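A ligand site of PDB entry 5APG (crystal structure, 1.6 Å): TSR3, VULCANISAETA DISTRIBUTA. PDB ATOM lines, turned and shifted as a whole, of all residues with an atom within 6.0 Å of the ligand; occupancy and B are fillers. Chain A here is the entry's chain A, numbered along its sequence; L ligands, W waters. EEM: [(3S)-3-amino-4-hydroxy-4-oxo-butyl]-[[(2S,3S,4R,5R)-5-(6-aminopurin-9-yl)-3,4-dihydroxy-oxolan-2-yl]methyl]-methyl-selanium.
Water W4 lies within hydrogen-bond range of O of Leu 45 (2.6 Å), O2' of the ligand (2.6 Å), NE2 of His 80 (2.7 Å) and N of Ile 69 (2.8 Å). Water W2 bridges the backbone NH (N) of Trp 73 and a nitrogen (N) of the ligand.
Leu 45 touches the ligand. Asp 46 touches the ligand (N to C2, 3.9 Å). N of Pro 47 touches C2 of the ligand, at 3.6 Å. Leu 68 touches the ligand. Asp 70 touches the ligand. Cys 71 touches the ligand. Ser 72 touches the ligand (O to CE, 3.9 Å). Trp 73 touches the ligand (CZ2 to C8, 3.5 Å). CB of Ala 76 touches CE of the ligand, 3.8 Å away. CE1 of His 80 touches O3' of the ligand, at 3.4 Å. Arg 92 touches the ligand (CA to N1, 3.9 Å). Leu 110 touches the ligand (O to C8, 3.4 Å). CB of Ser 111 touches O of the ligand, 3.4 Å away. CB of Ala 115 touches N9 of the ligand, at 3.4 Å. Within 4 Å of the ligand: Asn 18, Thr 19, Leu 45, Asp 46, Pro 47, Leu 68, Ile 69, Asp 70, Cys 71, Ser 72, Trp 73, Ala 76, His 80, Arg 92, Leu 93, Tyr 108, Leu 110, Ser 111, Thr 112 and Ala 115. Along chain A the residues within 4 Å of the ligand span positions 18 to 115.
N of Thr 112 sits at hydrogen-bond distance from OG1 of Thr 19 (3.4 Å). The side-chain hydroxyl (OG1) of Thr 19 sits at hydrogen-bond distance from the backbone NH (N) of Ile 113 (3.0 Å). O of Pro 47 lies within hydrogen-bond range of OH of Tyr 108, at 2.7 Å. N of Ala 20 lies within hydrogen-bond range of OD1 of Asn 18. A ring nitrogen (ND1) of His 80 lies within hydrogen-bond range of the backbone carbonyl oxygen (O) of Ala 76, at 2.8 Å. N of Leu 45 is in hydrogen-bond range of O of Ser 67, 3.1 Å away. O of Asp 46 sits close to N of Arg 92, 3.5 Å away. The backbone NH of Asp 46 is in hydrogen-bond range of the backbone carbonyl oxygen of Arg 91 (2.9 Å).
OXT of the ligand sits at hydrogen-bond distance from N of Thr 19, at 2.9 Å. An oxygen (O) of the ligand is in hydrogen-bond range of the side-chain hydroxyl (OG1) of Thr 19, 2.5 Å away. An oxygen (O3') of the ligand is in hydrogen-bond range of the backbone carbonyl oxygen (O) of Ile 69, 2.7 Å away. N of Thr 112 sits at hydrogen-bond distance from O of the ligand, 2.9 Å away. O of Tyr 108 is in hydrogen-bond range of N6 of the ligand. N of Leu 93 lies within hydrogen-bond range of N1 of the ligand (3.1 Å). The side-chain amide nitrogen (ND2) of Asn 18 is in hydrogen-bond range of an oxygen (OXT) of the ligand.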
ATOM      1  N   ASP A  13      35.118 -28.964 -28.626  1.00  0.00           N
ATOM      2  CA  ASP A  13      36.415 -29.126 -27.962  1.00  0.00           C
ATOM      3  C   ASP A  13      36.595 -30.558 -27.457  1.00  0.00           C
ATOM      4  O   ASP A  13      35.646 -31.330 -27.464  1.00  0.00           O
ATOM      5  CB  ASP A  13      36.526 -28.149 -26.785  1.00  0.00           C
ATOM      6  N   LYS A  17      39.126 -31.346 -21.299  1.00  0.00           N
ATOM      7  CA  LYS A  17      39.644 -30.036 -20.945  1.00  0.00           C
ATOM      8  C   LYS A  17      38.519 -29.008 -20.851  1.00  0.00           C
ATOM      9  O   LYS A  17      38.746 -27.828 -20.591  1.00  0.00           O
ATOM     10  CB  LYS A  17      40.696 -29.574 -21.960  1.00  0.00           C
ATOM     11  CG  LYS A  17      41.941 -30.439 -21.975  1.00  0.00           C
ATOM     12  CD  LYS A  17      42.986 -29.901 -22.950  1.00  0.00           C
ATOM     13  CE  LYS A  17      44.310 -30.639 -22.785  1.00  0.00           C
ATOM     14  NZ  LYS A  17      45.314 -30.207 -23.794  1.00  0.00           N
ATOM     15  N   ASN A  18      37.292 -29.475 -21.052  1.00  0.00           N
ATOM     16  CA  ASN A  18      36.110 -28.634 -21.006  1.00  0.00           C
ATOM     17  C   ASN A  18      35.566 -28.542 -19.579  1.00  0.00           C
ATOM     18  O   ASN A  18      35.451 -29.554 -18.893  1.00  0.00           O
ATOM     19  CB  ASN A  18      35.059 -29.176 -21.965  1.00  0.00           C
ATOM     20  CG  ASN A  18      33.751 -28.440 -21.872  1.00  0.00           C
ATOM     21  OD1 ASN A  18      32.853 -28.832 -21.119  1.00  0.00           O
ATOM     22  ND2 ASN A  18      33.613 -27.366 -22.629  1.00  0.00           N
ATOM     23  N   THR A  19      35.219 -27.331 -19.132  1.00  0.00           N
ATOM     24  CA  THR A  19      34.832 -27.152 -17.726  1.00  0.00           C
ATOM     25  C   THR A  19      33.381 -27.533 -17.475  1.00  0.00           C
ATOM     26  O   THR A  19      33.011 -27.850 -16.344  1.00  0.00           O
ATOM     27  CB  THR A  19      35.077 -25.700 -17.223  1.00  0.00           C
ATOM     28  OG1 THR A  19      34.174 -24.784 -17.867  1.00  0.00           O
ATOM     29  CG2 THR A  19      36.517 -25.270 -17.494  1.00  0.00           C
ATOM     30  N   ALA A  20      32.565 -27.524 -18.528  1.00  0.00           N
ATOM     31  CA  ALA A  20      31.163 -27.914 -18.398  1.00  0.00           C
ATOM     32  C   ALA A  20      31.045 -29.412 -18.126  1.00  0.00           C
ATOM     33  O   ALA A  20      30.228 -29.841 -17.313  1.00  0.00           O
ATOM     34  CB  ALA A  20      30.371 -27.525 -19.640  1.00  0.00           C
ATOM     35  N   LEU A  45      22.372 -17.706 -19.502  1.00  0.00           N
ATOM     36  CA  LEU A  45      23.558 -16.870 -19.652  1.00  0.00           C
ATOM     37  C   LEU A  45      23.792 -16.702 -21.141  1.00  0.00           C
ATOM     38  O   LEU A  45      23.675 -17.649 -21.926  1.00  0.00           O
ATOM     39  CB  LEU A  45      24.765 -17.478 -18.957  1.00  0.00           C
ATOM     40  CG  LEU A  45      24.657 -17.613 -17.426  1.00  0.00           C
ATOM     41  CD1 LEU A  45      25.986 -18.039 -16.834  1.00  0.00           C
ATOM     42  CD2 LEU A  45      24.184 -16.311 -16.791  1.00  0.00           C
ATOM     43  N   ASP A  46      24.111 -15.475 -21.535  1.00  0.00           N
ATOM     44  CA  ASP A  46      24.270 -15.149 -22.937  1.00  0.00           C
ATOM     45  C   ASP A  46      25.200 -13.947 -23.031  1.00  0.00           C
ATOM     46  O   ASP A  46      24.788 -12.828 -22.726  1.00  0.00           O
ATOM     47  CB  ASP A  46      22.914 -14.856 -23.591  1.00  0.00           C
ATOM     48  CG  ASP A  46      23.023 -14.610 -25.097  1.00  0.00           C
ATOM     49  OD1 ASP A  46      24.112 -14.280 -25.609  1.00  0.00           O
ATOM     50  OD2 ASP A  46      21.983 -14.738 -25.772  1.00  0.00           O
ATOM     51  N   PRO A  47      26.458 -14.180 -23.431  1.00  0.00           N
ATOM     52  CA  PRO A  47      27.435 -13.095 -23.512  1.00  0.00           C
ATOM     53  C   PRO A  47      27.167 -12.097 -24.639  1.00  0.00           C
ATOM     54  O   PRO A  47      27.824 -11.056 -24.664  1.00  0.00           O
ATOM     55  CB  PRO A  47      28.756 -13.839 -23.744  1.00  0.00           C
ATOM     56  CG  PRO A  47      28.346 -15.055 -24.510  1.00  0.00           C
ATOM     57  CD  PRO A  47      27.012 -15.457 -23.915  1.00  0.00           C
ATOM     58  N   SER A  67      20.134 -21.814 -17.298  1.00  0.00           N
ATOM     59  CA  SER A  67      20.561 -22.499 -18.512  1.00  0.00           C
ATOM     60  C   SER A  67      21.828 -21.891 -19.080  1.00  0.00           C
ATOM     61  O   SER A  67      22.089 -20.701 -18.909  1.00  0.00           O
ATOM     62  CB  SER A  67      19.440 -22.459 -19.557  1.00  0.00           C
ATOM     63  OG  SER A  67      18.273 -23.109 -19.103  1.00  0.00           O
ATOM     64  N   LEU A  68      22.623 -22.719 -19.760  1.00  0.00           N
ATOM     65  CA  LEU A  68      23.799 -22.246 -20.484  1.00  0.00           C
ATOM     66  C   LEU A  68      24.022 -23.072 -21.744  1.00  0.00           C
ATOM     67  O   LEU A  68      23.670 -24.242 -21.796  1.00  0.00           O
ATOM     68  CB  LEU A  68      25.067 -22.315 -19.624  1.00  0.00           C
ATOM     69  CG  LEU A  68      25.268 -21.479 -18.362  1.00  0.00           C
ATOM     70  CD1 LEU A  68      24.604 -22.113 -17.147  1.00  0.00           C
ATOM     71  CD2 LEU A  68      26.756 -21.275 -18.133  1.00  0.00           C
ATOM     72  N   ILE A  69      24.631 -22.437 -22.737  1.00  0.00           N
ATOM     73  CA  ILE A  69      25.137 -23.169 -23.886  1.00  0.00           C
ATOM     74  C   ILE A  69      26.652 -23.221 -23.789  1.00  0.00           C
ATOM     75  O   ILE A  69      27.312 -22.181 -23.662  1.00  0.00           O
ATOM     76  CB  ILE A  69      24.717 -22.504 -25.214  1.00  0.00           C
ATOM     77  CG1 ILE A  69      23.197 -22.568 -25.398  1.00  0.00           C
ATOM     78  CG2 ILE A  69      25.407 -23.194 -26.396  1.00  0.00           C
ATOM     79  CD1 ILE A  69      22.669 -21.665 -26.500  1.00  0.00           C
ATOM     80  N   ASP A  70      27.208 -24.424 -23.802  1.00  0.00           N
ATOM     81  CA  ASP A  70      28.654 -24.576 -23.793  1.00  0.00           C
ATOM     82  C   ASP A  70      29.150 -24.846 -25.219  1.00  0.00           C
ATOM     83  O   ASP A  70      28.763 -25.826 -25.844  1.00  0.00           O
ATOM     84  CB  ASP A  70      29.085 -25.723 -22.863  1.00  0.00           C
ATOM     85  CG  ASP A  70      30.588 -25.957 -22.881  1.00  0.00           C
ATOM     86  OD1 ASP A  70      31.308 -25.256 -22.149  1.00  0.00           O
ATOM     87  OD2 ASP A  70      31.043 -26.842 -23.621  1.00  0.00           O
ATOM     88  N   CYS A  71      30.004 -23.958 -25.710  1.00  0.00           N
ATOM     89  CA  CYS A  71      30.543 -24.082 -27.060  1.00  0.00           C
ATOM     90  C   CYS A  71      31.905 -23.396 -27.077  1.00  0.00           C
ATOM     91  O   CYS A  71      32.327 -22.871 -26.068  1.00  0.00           O
ATOM     92  CB  CYS A  71      29.601 -23.458 -28.084  1.00  0.00           C
ATOM     93  SG  CYS A  71      29.310 -21.679 -27.840  1.00  0.00           S
ATOM     94  N   SER A  72      32.587 -23.393 -28.216  1.00  0.00           N
ATOM     95  CA  SER A  72      33.842 -22.648 -28.306  1.00  0.00           C
ATOM     96  C   SER A  72      33.526 -21.162 -28.359  1.00  0.00           C
ATOM     97  O   SER A  72      32.456 -20.763 -28.820  1.00  0.00           O
ATOM     98  CB  SER A  72      34.648 -23.071 -29.531  1.00  0.00           C
ATOM     99  OG  SER A  72      34.030 -22.609 -30.717  1.00  0.00           O
ATOM    100  N   TRP A  73      34.454 -20.333 -27.883  1.00  0.00           N
ATOM    101  CA  TRP A  73      34.251 -18.885 -27.959  1.00  0.00           C
ATOM    102  C   TRP A  73      34.259 -18.400 -29.412  1.00  0.00           C
ATOM    103  O   TRP A  73      33.655 -17.378 -29.732  1.00  0.00           O
ATOM    104  CB  TRP A  73      35.307 -18.136 -27.139  1.00  0.00           C
ATOM    105  CG  TRP A  73      34.887 -17.962 -25.710  1.00  0.00           C
ATOM    106  CD1 TRP A  73      35.381 -18.627 -24.620  1.00  0.00           C
ATOM    107  CD2 TRP A  73      33.875 -17.076 -25.219  1.00  0.00           C
ATOM    108  NE1 TRP A  73      34.739 -18.202 -23.478  1.00  0.00           N
ATOM    109  CE2 TRP A  73      33.810 -17.246 -23.821  1.00  0.00           C
ATOM    110  CE3 TRP A  73      33.018 -16.151 -25.820  1.00  0.00           C
ATOM    111  CZ2 TRP A  73      32.929 -16.534 -23.018  1.00  0.00           C
ATOM    112  CZ3 TRP A  73      32.140 -15.430 -25.022  1.00  0.00           C
ATOM    113  CH2 TRP A  73      32.100 -15.632 -23.631  1.00  0.00           C
ATOM    114  N   ALA A  76      30.701 -18.801 -30.294  1.00  0.00           N
ATOM    115  CA  ALA A  76      29.740 -18.352 -29.296  1.00  0.00           C
ATOM    116  C   ALA A  76      28.752 -17.300 -29.809  1.00  0.00           C
ATOM    117  O   ALA A  76      27.558 -17.381 -29.526  1.00  0.00           O
ATOM    118  CB  ALA A  76      30.465 -17.823 -28.066  1.00  0.00           C
ATOM    119  N   HIS A  80      24.654 -18.160 -30.075  1.00  0.00           N
ATOM    120  CA  HIS A  80      23.700 -17.460 -29.214  1.00  0.00           C
ATOM    121  C   HIS A  80      22.771 -16.547 -30.007  1.00  0.00           C
ATOM    122  O   HIS A  80      21.601 -16.423 -29.677  1.00  0.00           O
ATOM    123  CB  HIS A  80      24.434 -16.649 -28.150  1.00  0.00           C
ATOM    124  CG  HIS A  80      25.021 -17.477 -27.049  1.00  0.00           C
ATOM    125  ND1 HIS A  80      26.262 -18.060 -27.137  1.00  0.00           N
ATOM    126  CD2 HIS A  80      24.513 -17.842 -25.846  1.00  0.00           C
ATOM    127  CE1 HIS A  80      26.503 -18.749 -26.034  1.00  0.00           C
ATOM    128  NE2 HIS A  80      25.465 -18.624 -25.228  1.00  0.00           N
ATOM    129  N   ARG A  91      20.567 -13.059 -20.151  1.00  0.00           N
ATOM    130  CA  ARG A  91      21.376 -12.132 -19.365  1.00  0.00           C
ATOM    131  C   ARG A  91      22.869 -12.364 -19.587  1.00  0.00           C
ATOM    132  O   ARG A  91      23.345 -13.504 -19.551  1.00  0.00           O
ATOM    133  CB  ARG A  91      21.060 -12.276 -17.867  1.00  0.00           C
ATOM    134  CG  ARG A  91      19.647 -11.894 -17.465  1.00  0.00           C
ATOM    135  CD  ARG A  91      19.383 -10.395 -17.687  1.00  0.00           C
ATOM    136  NE  ARG A  91      18.061  -9.982 -17.219  1.00  0.00           N
ATOM    137  CZ  ARG A  91      16.958  -9.970 -17.966  1.00  0.00           C
ATOM    138  NH1 ARG A  91      17.007 -10.345 -19.240  1.00  0.00           N
ATOM    139  NH2 ARG A  91      15.803  -9.579 -17.430  1.00  0.00           N
ATOM    140  N   ARG A  92      23.620 -11.293 -19.820  1.00  0.00           N
ATOM    141  CA  ARG A  92      25.072 -11.396 -19.799  1.00  0.00           C
ATOM    142  C   ARG A  92      25.516 -11.312 -18.357  1.00  0.00           C
ATOM    143  O   ARG A  92      24.755 -10.879 -17.490  1.00  0.00           O
ATOM    144  CB  ARG A  92      25.746 -10.294 -20.636  1.00  0.00           C
ATOM    145  CG  ARG A  92      25.557  -8.867 -20.095  1.00  0.00           C
ATOM    146  CD  ARG A  92      26.507  -7.904 -20.819  1.00  0.00           C
ATOM    147  NE  ARG A  92      26.360  -6.499 -20.407  1.00  0.00           N
ATOM    148  CZ  ARG A  92      26.997  -5.950 -19.381  1.00  0.00           C
ATOM    149  NH1 ARG A  92      27.813  -6.673 -18.625  1.00  0.00           N
ATOM    150  NH2 ARG A  92      26.809  -4.669 -19.094  1.00  0.00           N
ATOM    151  N   LEU A  93      26.748 -11.721 -18.085  1.00  0.00           N
ATOM    152  CA  LEU A  93      27.304 -11.486 -16.773  1.00  0.00           C
ATOM    153  C   LEU A  93      27.853 -10.072 -16.724  1.00  0.00           C
ATOM    154  O   LEU A  93      28.334  -9.561 -17.735  1.00  0.00           O
ATOM    155  CB  LEU A  93      28.407 -12.489 -16.443  1.00  0.00           C
ATOM    156  CG  LEU A  93      27.924 -13.914 -16.155  1.00  0.00           C
ATOM    157  CD1 LEU A  93      29.112 -14.836 -16.128  1.00  0.00           C
ATOM    158  CD2 LEU A  93      27.146 -13.965 -14.848  1.00  0.00           C
ATOM    159  N   PRO A  94      27.781  -9.423 -15.551  1.00  0.00           N
ATOM    160  CA  PRO A  94      28.504  -8.170 -15.364  1.00  0.00           C
ATOM    161  C   PRO A  94      29.992  -8.421 -15.530  1.00  0.00           C
ATOM    162  O   PRO A  94      30.443  -9.569 -15.400  1.00  0.00           O
ATOM    163  CB  PRO A  94      28.149  -7.759 -13.923  1.00  0.00           C
ATOM    164  CG  PRO A  94      27.638  -8.975 -13.280  1.00  0.00           C
ATOM    165  CD  PRO A  94      27.002  -9.797 -14.365  1.00  0.00           C
ATOM    166  N   TYR A 108      35.781 -10.308 -19.104  1.00  0.00           N
ATOM    167  CA  TYR A 108      34.531 -10.733 -19.727  1.00  0.00           C
ATOM    168  C   TYR A 108      34.508 -12.165 -20.269  1.00  0.00           C
ATOM    169  O   TYR A 108      33.493 -12.852 -20.144  1.00  0.00           O
ATOM    170  CB  TYR A 108      34.144  -9.778 -20.864  1.00  0.00           C
ATOM    171  CG  TYR A 108      32.686  -9.873 -21.263  1.00  0.00           C
ATOM    172  CD1 TYR A 108      31.689  -9.567 -20.352  1.00  0.00           C
ATOM    173  CD2 TYR A 108      32.322 -10.273 -22.538  1.00  0.00           C
ATOM    174  CE1 TYR A 108      30.354  -9.638 -20.704  1.00  0.00           C
ATOM    175  CE2 TYR A 108      30.980 -10.358 -22.899  1.00  0.00           C
ATOM    176  CZ  TYR A 108      30.005 -10.047 -21.967  1.00  0.00           C
ATOM    177  OH  TYR A 108      28.671 -10.118 -22.319  1.00  0.00           O
ATOM    178  N   ILE A 109      35.593 -12.600 -20.890  1.00  0.00           N
ATOM    179  CA  ILE A 109      35.611 -13.908 -21.532  1.00  0.00           C
ATOM    180  C   ILE A 109      35.902 -15.009 -20.522  1.00  0.00           C
ATOM    181  O   ILE A 109      37.063 -15.350 -20.285  1.00  0.00           O
ATOM    182  CB  ILE A 109      36.645 -13.951 -22.685  1.00  0.00           C
ATOM    183  CG1 ILE A 109      36.406 -12.793 -23.663  1.00  0.00           C
ATOM    184  CG2 ILE A 109      36.615 -15.298 -23.390  1.00  0.00           C
ATOM    185  CD1 ILE A 109      35.008 -12.782 -24.267  1.00  0.00           C
ATOM    186  N   LEU A 110      34.850 -15.572 -19.936  1.00  0.00           N
ATOM    187  CA  LEU A 110      35.007 -16.541 -18.854  1.00  0.00           C
ATOM    188  C   LEU A 110      34.823 -17.980 -19.321  1.00  0.00           C
ATOM    189  O   LEU A 110      34.168 -18.234 -20.323  1.00  0.00           O
ATOM    190  CB  LEU A 110      34.002 -16.248 -17.728  1.00  0.00           C
ATOM    191  CG  LEU A 110      33.956 -14.805 -17.226  1.00  0.00           C
ATOM    192  CD1 LEU A 110      32.935 -14.664 -16.097  1.00  0.00           C
ATOM    193  CD2 LEU A 110      35.335 -14.328 -16.768  1.00  0.00           C
ATOM    194  N   SER A 111      35.405 -18.919 -18.573  1.00  0.00           N
ATOM    195  CA  SER A 111      35.102 -20.326 -18.779  1.00  0.00           C
ATOM    196  C   SER A 111      33.668 -20.592 -18.335  1.00  0.00           C
ATOM    197  O   SER A 111      33.081 -19.790 -17.601  1.00  0.00           O
ATOM    198  CB  SER A 111      36.072 -21.222 -18.001  1.00  0.00           C
ATOM    199  OG  SER A 111      35.865 -21.122 -16.600  1.00  0.00           O
ATOM    200  N   THR A 112      33.103 -21.699 -18.789  1.00  0.00           N
ATOM    201  CA  THR A 112      31.742 -22.042 -18.428  1.00  0.00           C
ATOM    202  C   THR A 112      31.605 -22.162 -16.906  1.00  0.00           C
ATOM    203  O   THR A 112      30.635 -21.689 -16.313  1.00  0.00           O
ATOM    204  CB  THR A 112      31.290 -23.346 -19.114  1.00  0.00           C
ATOM    205  OG1 THR A 112      31.280 -23.147 -20.540  1.00  0.00           O
ATOM    206  CG2 THR A 112      29.881 -23.746 -18.658  1.00  0.00           C
ATOM    207  N   ILE A 113      32.598 -22.772 -16.252  1.00  0.00           N
ATOM    208  CA  ILE A 113      32.498 -22.969 -14.807  1.00  0.00           C
ATOM    209  C   ILE A 113      32.611 -21.650 -14.045  1.00  0.00           C
ATOM    210  O   ILE A 113      31.933 -21.456 -13.040  1.00  0.00           O
ATOM    211  CB  ILE A 113      33.561 -23.990 -14.287  1.00  0.00           C
ATOM    212  CG1 ILE A 113      33.273 -24.350 -12.830  1.00  0.00           C
ATOM    213  CG2 ILE A 113      34.990 -23.462 -14.419  1.00  0.00           C
ATOM    214  CD1 ILE A 113      34.009 -25.594 -12.333  1.00  0.00           C
ATOM    215  N   ALA A 115      31.617 -18.784 -15.242  1.00  0.00           N
ATOM    216  CA  ALA A 115      30.359 -18.115 -15.498  1.00  0.00           C
ATOM    217  C   ALA A 115      29.250 -18.624 -14.595  1.00  0.00           C
ATOM    218  O   ALA A 115      28.464 -17.832 -14.067  1.00  0.00           O
ATOM    219  CB  ALA A 115      29.965 -18.285 -16.929  1.00  0.00           C
ATOM    220  N   VAL A 116      29.185 -19.944 -14.423  1.00  0.00           N
ATOM    221  CA  VAL A 116      28.208 -20.541 -13.520  1.00  0.00           C
ATOM    222  C   VAL A 116      28.428 -20.023 -12.107  1.00  0.00           C
ATOM    223  O   VAL A 116      27.485 -19.599 -11.435  1.00  0.00           O
ATOM    224  CB  VAL A 116      28.282 -22.080 -13.543  1.00  0.00           C
ATOM    225  CG1 VAL A 116      27.502 -22.690 -12.386  1.00  0.00           C
ATOM    226  CG2 VAL A 116      27.781 -22.612 -14.887  1.00  0.00           C
HETATM  227  C2  EEM L   1      27.510 -14.511 -20.000  1.00  0.00           C
HETATM  228  N3  EEM L   1      27.826 -15.773 -20.097  1.00  0.00           N
HETATM  229  C4  EEM L   1      29.093 -16.142 -20.117  1.00  0.00           C
HETATM  230  C1' EEM L   1      29.077 -18.659 -20.222  1.00  0.00           C
HETATM  231  C2' EEM L   1      28.332 -18.744 -21.574  1.00  0.00           C
HETATM  232  C3' EEM L   1      29.303 -19.319 -22.397  1.00  0.00           C
HETATM  233  C4' EEM L   1      30.043 -20.193 -21.694  1.00  0.00           C
HETATM  234  C5' EEM L   1      31.485 -20.205 -22.028  1.00  0.00           C
HETATM  235  O   EEM L   1      34.779 -23.666 -20.019  1.00  0.00           O
HETATM  236  C   EEM L   1      35.251 -24.067 -21.046  1.00  0.00           C
HETATM  237  OXT EEM L   1      35.653 -25.209 -21.132  1.00  0.00           O
HETATM  238  CA  EEM L   1      35.309 -23.168 -22.271  1.00  0.00           C
HETATM  239  N   EEM L   1      36.089 -23.833 -23.273  1.00  0.00           N
HETATM  240  CB  EEM L   1      33.862 -22.955 -22.700  1.00  0.00           C
HETATM  241  CG  EEM L   1      33.659 -21.820 -23.685  1.00  0.00           C
HETATM  242 SE   EEM L   1      31.777 -21.209 -23.678  1.00  0.00          SE
HETATM  243  CE  EEM L   1      31.475 -19.945 -25.108  1.00  0.00           C
HETATM  244  O4' EEM L   1      29.992 -19.541 -20.226  1.00  0.00           O
HETATM  245  O3' EEM L   1      28.730 -19.832 -23.661  1.00  0.00           O
HETATM  246  O2' EEM L   1      27.318 -19.713 -21.303  1.00  0.00           O
HETATM  247  N9  EEM L   1      29.731 -17.319 -20.205  1.00  0.00           N
HETATM  248  C8  EEM L   1      31.019 -17.044 -20.177  1.00  0.00           C
HETATM  249  N7  EEM L   1      31.231 -15.755 -20.085  1.00  0.00           N
HETATM  250  C5  EEM L   1      30.045 -15.137 -20.040  1.00  0.00           C
HETATM  251  N1  EEM L   1      28.376 -13.524 -19.930  1.00  0.00           N
HETATM  252  C6  EEM L   1      29.652 -13.767 -19.941  1.00  0.00           C
HETATM  253  N6  EEM L   1      30.601 -12.736 -19.880  1.00  0.00           N
HETATM  254  O   HOH W   1      37.960 -21.153 -24.122  1.00  0.00           O
HETATM  255  O   HOH W   2      36.735 -21.885 -26.082  1.00  0.00           O
HETATM  256  O   HOH W   3      39.165 -25.033 -22.826  1.00  0.00           O
HETATM  257  O   HOH W   4      25.106 -19.649 -22.759  1.00  0.00           O
